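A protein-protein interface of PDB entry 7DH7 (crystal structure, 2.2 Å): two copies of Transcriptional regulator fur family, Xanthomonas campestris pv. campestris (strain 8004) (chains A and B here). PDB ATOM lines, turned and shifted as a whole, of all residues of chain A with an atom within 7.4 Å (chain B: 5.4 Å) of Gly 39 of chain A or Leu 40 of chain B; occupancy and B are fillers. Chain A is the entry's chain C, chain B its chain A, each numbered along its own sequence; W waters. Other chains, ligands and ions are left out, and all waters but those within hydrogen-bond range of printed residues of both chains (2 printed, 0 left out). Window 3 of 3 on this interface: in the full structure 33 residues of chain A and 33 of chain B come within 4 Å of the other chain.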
ATOM      1  N   ARG A  33      11.955  -2.759   0.731  1.00  0.00           N
ATOM      2  CA  ARG A  33      12.267  -2.557  -0.685  1.00  0.00           C
ATOM      3  C   ARG A  33      11.063  -2.864  -1.562  1.00  0.00           C
ATOM      4  O   ARG A  33      10.757  -2.110  -2.498  1.00  0.00           O
ATOM      5  CB  ARG A  33      13.451  -3.421  -1.115  1.00  0.00           C
ATOM      6  CG  ARG A  33      13.850  -3.244  -2.582  1.00  0.00           C
ATOM      7  CD  ARG A  33      14.937  -4.229  -2.986  1.00  0.00           C
ATOM      8  NE  ARG A  33      15.612  -4.755  -1.813  1.00  0.00           N
ATOM      9  CZ  ARG A  33      15.567  -6.036  -1.455  1.00  0.00           C
ATOM     10  NH1 ARG A  33      14.886  -6.903  -2.194  1.00  0.00           N
ATOM     11  NH2 ARG A  33      16.187  -6.449  -0.357  1.00  0.00           N
ATOM     12  N   ALA A  34      10.339  -3.945  -1.245  1.00  0.00           N
ATOM     13  CA  ALA A  34       9.140  -4.286  -2.009  1.00  0.00           C
ATOM     14  C   ALA A  34       8.081  -3.191  -1.900  1.00  0.00           C
ATOM     15  O   ALA A  34       7.393  -2.882  -2.885  1.00  0.00           O
ATOM     16  CB  ALA A  34       8.573  -5.632  -1.545  1.00  0.00           C
ATOM     17  N   CYS A  35       7.929  -2.594  -0.711  1.00  0.00           N
ATOM     18  CA  CYS A  35       6.996  -1.478  -0.520  1.00  0.00           C
ATOM     19  C   CYS A  35       7.336  -0.320  -1.458  1.00  0.00           C
ATOM     20  O   CYS A  35       6.445   0.364  -1.970  1.00  0.00           O
ATOM     21  CB  CYS A  35       7.014  -1.008   0.938  1.00  0.00           C
ATOM     22  SG  CYS A  35       5.765  -1.840   1.992  1.00  0.00           S
ATOM     23  N   SER A  36       8.631  -0.056  -1.611  1.00  0.00           N
ATOM     24  CA  SER A  36       9.093   1.003  -2.498  1.00  0.00           C
ATOM     25  C   SER A  36       8.734   0.712  -3.951  1.00  0.00           C
ATOM     26  O   SER A  36       8.303   1.614  -4.681  1.00  0.00           O
ATOM     27  CB  SER A  36      10.594   1.196  -2.341  1.00  0.00           C
ATOM     28  OG  SER A  36      10.890   1.815  -1.097  1.00  0.00           O
ATOM     29  N   GLU A  37       8.929  -0.530  -4.387  1.00  0.00           N
ATOM     30  CA  GLU A  37       8.643  -0.850  -5.781  1.00  0.00           C
ATOM     31  C   GLU A  37       7.149  -1.006  -6.052  1.00  0.00           C
ATOM     32  O   GLU A  37       6.705  -0.768  -7.178  1.00  0.00           O
ATOM     33  CB  GLU A  37       9.444  -2.093  -6.218  1.00  0.00           C
ATOM     34  CG  GLU A  37       8.845  -3.461  -5.910  1.00  0.00           C
ATOM     35  CD  GLU A  37       9.328  -4.573  -6.875  1.00  0.00           C
ATOM     36  OE1 GLU A  37      10.097  -4.279  -7.815  1.00  0.00           O
ATOM     37  OE2 GLU A  37       8.930  -5.748  -6.699  1.00  0.00           O
ATOM     38  N   ARG A  38       6.347  -1.307  -5.037  1.00  0.00           N
ATOM     39  CA  ARG A  38       4.921  -1.514  -5.231  1.00  0.00           C
ATOM     40  C   ARG A  38       4.061  -0.269  -5.078  1.00  0.00           C
ATOM     41  O   ARG A  38       2.918  -0.298  -5.542  1.00  0.00           O
ATOM     42  CB  ARG A  38       4.392  -2.556  -4.239  1.00  0.00           C
ATOM     43  CG  ARG A  38       4.924  -3.969  -4.483  1.00  0.00           C
ATOM     44  CD  ARG A  38       4.285  -4.915  -3.475  1.00  0.00           C
ATOM     45  NE  ARG A  38       5.014  -6.170  -3.340  1.00  0.00           N
ATOM     46  CZ  ARG A  38       4.532  -7.220  -2.703  1.00  0.00           C
ATOM     47  NH1 ARG A  38       3.314  -7.160  -2.170  1.00  0.00           N
ATOM     48  NH2 ARG A  38       5.264  -8.316  -2.595  1.00  0.00           N
ATOM     49  N   GLY A  39       4.538   0.792  -4.395  1.00  0.00           N
ATOM     50  CA  GLY A  39       3.657   1.889  -4.026  1.00  0.00           C
ATOM     51  C   GLY A  39       2.960   1.718  -2.684  1.00  0.00           C
ATOM     52  O   GLY A  39       1.768   2.020  -2.557  1.00  0.00           O
ATOM     53  N   LEU A  40       3.668   1.215  -1.670  1.00  0.00           N
ATOM     54  CA  LEU A  40       3.086   0.983  -0.348  1.00  0.00           C
ATOM     55  C   LEU A  40       3.844   1.771   0.715  1.00  0.00           C
ATOM     56  O   LEU A  40       5.059   1.965   0.618  1.00  0.00           O
ATOM     57  CB  LEU A  40       3.104  -0.518   0.013  1.00  0.00           C
ATOM     58  CG  LEU A  40       2.207  -1.471  -0.798  1.00  0.00           C
ATOM     59  CD1 LEU A  40       2.608  -2.861  -0.473  1.00  0.00           C
ATOM     60  CD2 LEU A  40       0.741  -1.289  -0.452  1.00  0.00           C
ATOM     61  N   ARG A  41       3.124   2.216   1.738  1.00  0.00           N
ATOM     62  CA  ARG A  41       3.725   2.905   2.875  1.00  0.00           C
ATOM     63  C   ARG A  41       3.972   1.934   4.023  1.00  0.00           C
ATOM     64  O   ARG A  41       3.043   1.266   4.503  1.00  0.00           O
ATOM     65  CB  ARG A  41       2.817   4.024   3.381  1.00  0.00           C
ATOM     66  CG  ARG A  41       3.007   5.358   2.716  1.00  0.00           C
ATOM     67  CD  ARG A  41       2.003   6.319   3.303  1.00  0.00           C
ATOM     68  NE  ARG A  41       1.992   6.251   4.760  1.00  0.00           N
ATOM     69  CZ  ARG A  41       1.170   6.960   5.524  1.00  0.00           C
ATOM     70  NH1 ARG A  41       0.298   7.782   4.960  1.00  0.00           N
ATOM     71  NH2 ARG A  41       1.220   6.850   6.840  1.00  0.00           N
ATOM     72  N   PHE A  89      -2.855  -5.104   6.665  1.00  0.00           N
ATOM     73  CA  PHE A  89      -1.976  -4.568   5.630  1.00  0.00           C
ATOM     74  C   PHE A  89      -0.960  -5.604   5.203  1.00  0.00           C
ATOM     75  O   PHE A  89      -0.756  -5.839   4.009  1.00  0.00           O
ATOM     76  CB  PHE A  89      -1.246  -3.312   6.134  1.00  0.00           C
ATOM     77  CG  PHE A  89       0.002  -2.953   5.325  1.00  0.00           C
ATOM     78  CD1 PHE A  89      -0.086  -2.118   4.223  1.00  0.00           C
ATOM     79  CD2 PHE A  89       1.253  -3.448   5.671  1.00  0.00           C
ATOM     80  CE1 PHE A  89       1.043  -1.789   3.467  1.00  0.00           C
ATOM     81  CE2 PHE A  89       2.374  -3.134   4.917  1.00  0.00           C
ATOM     82  CZ  PHE A  89       2.271  -2.294   3.805  1.00  0.00           C
ATOM     83  N   ASN A  93      -1.069  -7.798   1.520  1.00  0.00           N
ATOM     84  CA  ASN A  93       0.061  -7.635   0.624  1.00  0.00           C
ATOM     85  C   ASN A  93       0.951  -8.861   0.561  1.00  0.00           C
ATOM     86  O   ASN A  93       1.983  -8.816  -0.118  1.00  0.00           O
ATOM     87  CB  ASN A  93       0.859  -6.409   1.033  1.00  0.00           C
ATOM     88  CG  ASN A  93       0.175  -5.150   0.612  1.00  0.00           C
ATOM     89  OD1 ASN A  93       0.006  -4.914  -0.583  1.00  0.00           O
ATOM     90  ND2 ASN A  93      -0.289  -4.364   1.580  1.00  0.00           N
ATOM     91  N   ALA B  34      -8.496  -5.725  -4.848  1.00  0.00           N
ATOM     92  CA  ALA B  34      -7.213  -5.974  -4.205  1.00  0.00           C
ATOM     93  C   ALA B  34      -6.533  -4.662  -3.805  1.00  0.00           C
ATOM     94  O   ALA B  34      -6.036  -4.526  -2.683  1.00  0.00           O
ATOM     95  CB  ALA B  34      -6.321  -6.808  -5.127  1.00  0.00           C
ATOM     96  N   CYS B  35      -6.543  -3.661  -4.692  1.00  0.00           N
ATOM     97  CA  CYS B  35      -5.860  -2.402  -4.378  1.00  0.00           C
ATOM     98  C   CYS B  35      -6.489  -1.696  -3.180  1.00  0.00           C
ATOM     99  O   CYS B  35      -5.783  -1.136  -2.322  1.00  0.00           O
ATOM    100  CB  CYS B  35      -5.859  -1.495  -5.603  1.00  0.00           C
ATOM    101  SG  CYS B  35      -4.776  -2.071  -6.933  1.00  0.00           S
ATOM    102  N   SER B  36      -7.818  -1.708  -3.108  1.00  0.00           N
ATOM    103  CA  SER B  36      -8.539  -1.182  -1.952  1.00  0.00           C
ATOM    104  C   SER B  36      -8.082  -1.844  -0.666  1.00  0.00           C
ATOM    105  O   SER B  36      -7.797  -1.161   0.327  1.00  0.00           O
ATOM    106  CB  SER B  36     -10.037  -1.382  -2.138  1.00  0.00           C
ATOM    107  OG  SER B  36     -10.720  -0.751  -1.081  1.00  0.00           O
ATOM    108  N   ARG B  38      -5.345  -3.484  -0.058  1.00  0.00           N
ATOM    109  CA  ARG B  38      -3.922  -3.404   0.243  1.00  0.00           C
ATOM    110  C   ARG B  38      -3.429  -1.992   0.534  1.00  0.00           C
ATOM    111  O   ARG B  38      -2.286  -1.834   0.981  1.00  0.00           O
ATOM    112  CB  ARG B  38      -3.100  -3.971  -0.911  1.00  0.00           C
ATOM    113  CG  ARG B  38      -3.423  -5.394  -1.249  1.00  0.00           C
ATOM    114  CD  ARG B  38      -2.503  -5.881  -2.363  1.00  0.00           C
ATOM    115  NE  ARG B  38      -3.005  -7.108  -2.940  1.00  0.00           N
ATOM    116  CZ  ARG B  38      -2.414  -7.789  -3.914  1.00  0.00           C
ATOM    117  NH1 ARG B  38      -1.266  -7.370  -4.433  1.00  0.00           N
ATOM    118  NH2 ARG B  38      -2.987  -8.892  -4.374  1.00  0.00           N
ATOM    119  N   GLY B  39      -4.254  -0.976   0.307  1.00  0.00           N
ATOM    120  CA  GLY B  39      -3.792   0.397   0.362  1.00  0.00           C
ATOM    121  C   GLY B  39      -3.061   0.892  -0.869  1.00  0.00           C
ATOM    122  O   GLY B  39      -2.303   1.853  -0.770  1.00  0.00           O
ATOM    123  N   LEU B  40      -3.258   0.268  -2.021  1.00  0.00           N
ATOM    124  CA  LEU B  40      -2.603   0.683  -3.257  1.00  0.00           C
ATOM    125  C   LEU B  40      -3.468   1.693  -3.993  1.00  0.00           C
ATOM    126  O   LEU B  40      -4.694   1.682  -3.893  1.00  0.00           O
ATOM    127  CB  LEU B  40      -2.355  -0.501  -4.176  1.00  0.00           C
ATOM    128  CG  LEU B  40      -1.356  -1.584  -3.761  1.00  0.00           C
ATOM    129  CD1 LEU B  40      -1.522  -2.774  -4.705  1.00  0.00           C
ATOM    130  CD2 LEU B  40       0.068  -1.063  -3.789  1.00  0.00           C
ATOM    131  N   ARG B  41      -2.821   2.526  -4.795  1.00  0.00           N
ATOM    132  CA  ARG B  41      -3.479   3.674  -5.396  1.00  0.00           C
ATOM    133  C   ARG B  41      -3.498   3.519  -6.912  1.00  0.00           C
ATOM    134  O   ARG B  41      -2.449   3.313  -7.543  1.00  0.00           O
ATOM    135  CB  ARG B  41      -2.763   4.940  -4.939  1.00  0.00           C
ATOM    136  CG  ARG B  41      -3.070   6.184  -5.684  1.00  0.00           C
ATOM    137  CD  ARG B  41      -2.391   7.362  -4.978  1.00  0.00           C
ATOM    138  NE  ARG B  41      -3.033   7.644  -3.699  1.00  0.00           N
ATOM    139  CZ  ARG B  41      -2.718   8.666  -2.927  1.00  0.00           C
ATOM    140  NH1 ARG B  41      -1.755   9.493  -3.311  1.00  0.00           N
ATOM    141  NH2 ARG B  41      -3.361   8.860  -1.778  1.00  0.00           N
ATOM    142  N   LEU B  42      -4.690   3.591  -7.499  1.00  0.00           N
ATOM    143  CA  LEU B  42      -4.826   3.553  -8.952  1.00  0.00           C
ATOM    144  C   LEU B  42      -4.964   4.995  -9.456  1.00  0.00           C
ATOM    145  O   LEU B  42      -6.054   5.570  -9.508  1.00  0.00           O
ATOM    146  CB  LEU B  42      -5.995   2.667  -9.376  1.00  0.00           C
ATOM    147  CG  LEU B  42      -5.791   1.167  -9.153  1.00  0.00           C
ATOM    148  CD1 LEU B  42      -7.091   0.394  -9.359  1.00  0.00           C
ATOM    149  CD2 LEU B  42      -4.717   0.630 -10.065  1.00  0.00           C
ATOM    150  N   PHE B  89       4.164  -1.140 -11.819  1.00  0.00           N
ATOM    151  CA  PHE B  89       3.298  -1.149 -10.652  1.00  0.00           C
ATOM    152  C   PHE B  89       2.419  -2.391 -10.647  1.00  0.00           C
ATOM    153  O   PHE B  89       2.321  -3.079  -9.624  1.00  0.00           O
ATOM    154  CB  PHE B  89       2.460   0.150 -10.614  1.00  0.00           C
ATOM    155  CG  PHE B  89       1.250   0.094  -9.710  1.00  0.00           C
ATOM    156  CD1 PHE B  89       0.005  -0.379 -10.163  1.00  0.00           C
ATOM    157  CD2 PHE B  89       1.366   0.488  -8.386  1.00  0.00           C
ATOM    158  CE1 PHE B  89      -1.101  -0.413  -9.314  1.00  0.00           C
ATOM    159  CE2 PHE B  89       0.268   0.466  -7.540  1.00  0.00           C
ATOM    160  CZ  PHE B  89      -0.969   0.002  -7.999  1.00  0.00           C
ATOM    161  N   ASN B  93       3.039  -5.728  -7.927  1.00  0.00           N
ATOM    162  CA  ASN B  93       1.954  -6.135  -7.048  1.00  0.00           C
ATOM    163  C   ASN B  93       1.314  -7.432  -7.488  1.00  0.00           C
ATOM    164  O   ASN B  93       0.295  -7.813  -6.918  1.00  0.00           O
ATOM    165  CB  ASN B  93       0.889  -5.039  -6.961  1.00  0.00           C
ATOM    166  CG  ASN B  93       1.404  -3.816  -6.218  1.00  0.00           C
ATOM    167  OD1 ASN B  93       1.657  -3.879  -5.024  1.00  0.00           O
ATOM    168  ND2 ASN B  93       1.604  -2.720  -6.931  1.00  0.00           N
ATOM    169  N   PHE B  95      -0.271  -8.309 -10.228  1.00  0.00           N
ATOM    170  CA  PHE B  95      -1.465  -8.342 -11.062  1.00  0.00           C
ATOM    171  C   PHE B  95      -1.151  -8.704 -12.500  1.00  0.00           C
ATOM    172  O   PHE B  95      -2.056  -9.140 -13.223  1.00  0.00           O
ATOM    173  CB  PHE B  95      -2.190  -6.982 -11.038  1.00  0.00           C
ATOM    174  CG  PHE B  95      -2.568  -6.517  -9.656  1.00  0.00           C
ATOM    175  CD1 PHE B  95      -3.281  -7.354  -8.805  1.00  0.00           C
ATOM    176  CD2 PHE B  95      -2.221  -5.239  -9.214  1.00  0.00           C
ATOM    177  CE1 PHE B  95      -3.617  -6.956  -7.543  1.00  0.00           C
ATOM    178  CE2 PHE B  95      -2.578  -4.826  -7.953  1.00  0.00           C
ATOM    179  CZ  PHE B  95      -3.283  -5.688  -7.111  1.00  0.00           C
HETATM  180  O   HOH W   1       0.033   2.633  -4.510  1.00  0.00           O
HETATM  181  O   HOH W   2       0.848  -5.641  -2.979  1.00  0.00           O
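Arg 38 of chain A touches Leu 40 of chain B, and with the chains exchanged Leu 40 of chain A touches Arg 38 of chain B. Arg 38 of chain A touches Phe 89 of chain B, and with the chains exchanged Phe 89 of chain A touches Arg 38 of chain B. Arg 38 of chain A touches Asn 93 of chain B, and with the chains exchanged Asn 93 of chain A touches Arg 38 of chain B. Leu 40 of chain B touches its own counterpart, Leu 40 of chain A. Positions printed for both chains: 34, 35, 36, 38, 39, 40, 41, 89 and 93. Of the 8 pairs that touch across the chains among the printed residues, 7 have their exchanged pair printed and touching as well.
ND2 of Asn 93 of chain A sits at hydrogen-bond distance from O of Arg 38 of chain B (3.3 Å). The backbone carbonyl oxygen (O) of Arg 38 of chain A sits at hydrogen-bond distance from the side-chain amide nitrogen (ND2) of Asn 93 of chain B (3.1 Å).
Of chain B, only Leu 40 comes within 4 Å of Gly 39 of chain A. Gly 39 of chain B touches none of the printed residues of chain A. Of the printed residues of chain A, Phe 89 of chain B touches Arg 38. Of the printed residues of chain B, Leu 40 of chain A touches Arg 38 and Leu 40. Of the printed residues of chain A, Arg 38 of chain B touches Leu 40 (3.4 Å), Phe 89 (3.9 Å) and Asn 93 (3.2 Å). Printed residues of chain B within 4 Å of Arg 38 of chain A: Leu 40 (3.4 Å), Phe 89 (3.3 Å) and Asn 93 (3.1 Å). Of the printed residues of chain B, Phe 89 of chain A touches Arg 38 (3.9 Å). Ser 36 of chain A touches none of the printed residues of chain B. Glu 37 of chain A touches none of the printed residues of chain B. The nearest residue of chain B that does not touch Gly 39 of chain A is Gly 39 of chain B (4.4 Å).
Water W2 lies within hydrogen-bond range of OD1 of Asn 93 of chain A (2.6 Å), OD1 of Asn 93 of chain B (2.8 Å), NH1 of Arg 38 of chain A (3.0 Å) and NH1 of Arg 38 of chain B (3.1 Å). Water W1 bridges O of Gly 39 of chain A (2.7 Å) and N of Arg 41 of chain B (2.9 Å).
Printed residues of chain B that touch a printed residue of chain A: Arg 38, Leu 40, Phe 89 and Asn 93. Hydrophobic or aromatic side chains of chain B within 4 Å of the printed part of chain A: Leu 40 and Phe 89. Hydrophobic or aromatic side chains of chain A within 4 Å of the printed part of chain B: Leu 40 and Phe 89.
N of Leu 40 of chain B is in hydrogen-bond range of O of Cys 35 of chain B (2.9 Å). The guanidinium group (NH1) of Arg 38 of chain B is in hydrogen-bond range of the backbone carbonyl oxygen (O) of Asn 93 of chain B, 3.0 Å away. O of Phe 89 of chain B lies within hydrogen-bond range of ND2 of Asn 93 of chain B (2.8 Å). The backbone carbonyl oxygen (O) of Cys 35 of chain A is in hydrogen-bond range of the backbone NH (N) of Leu 40 of chain A (2.9 Å). O of Asn 93 of chain A is in hydrogen-bond range of NH1 of Arg 38 of chain A (3.0 Å). ND2 of Asn 93 of chain A lies within hydrogen-bond range of O of Phe 89 of chain A (2.9 Å).
Leu 40 of chain B touches Arg 38 of chain A. Phe 89 of chain B touches Arg 38 of chain A. Gly 39 of chain A touches Leu 40 of chain B. Arg 38 of chain B touches Leu 40 of chain A. CD2 of Leu 40 of chain B touches CD2 of Leu 40 of chain A, at 3.4 Å. Phe 89 of chain A touches Arg 38 of chain B.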
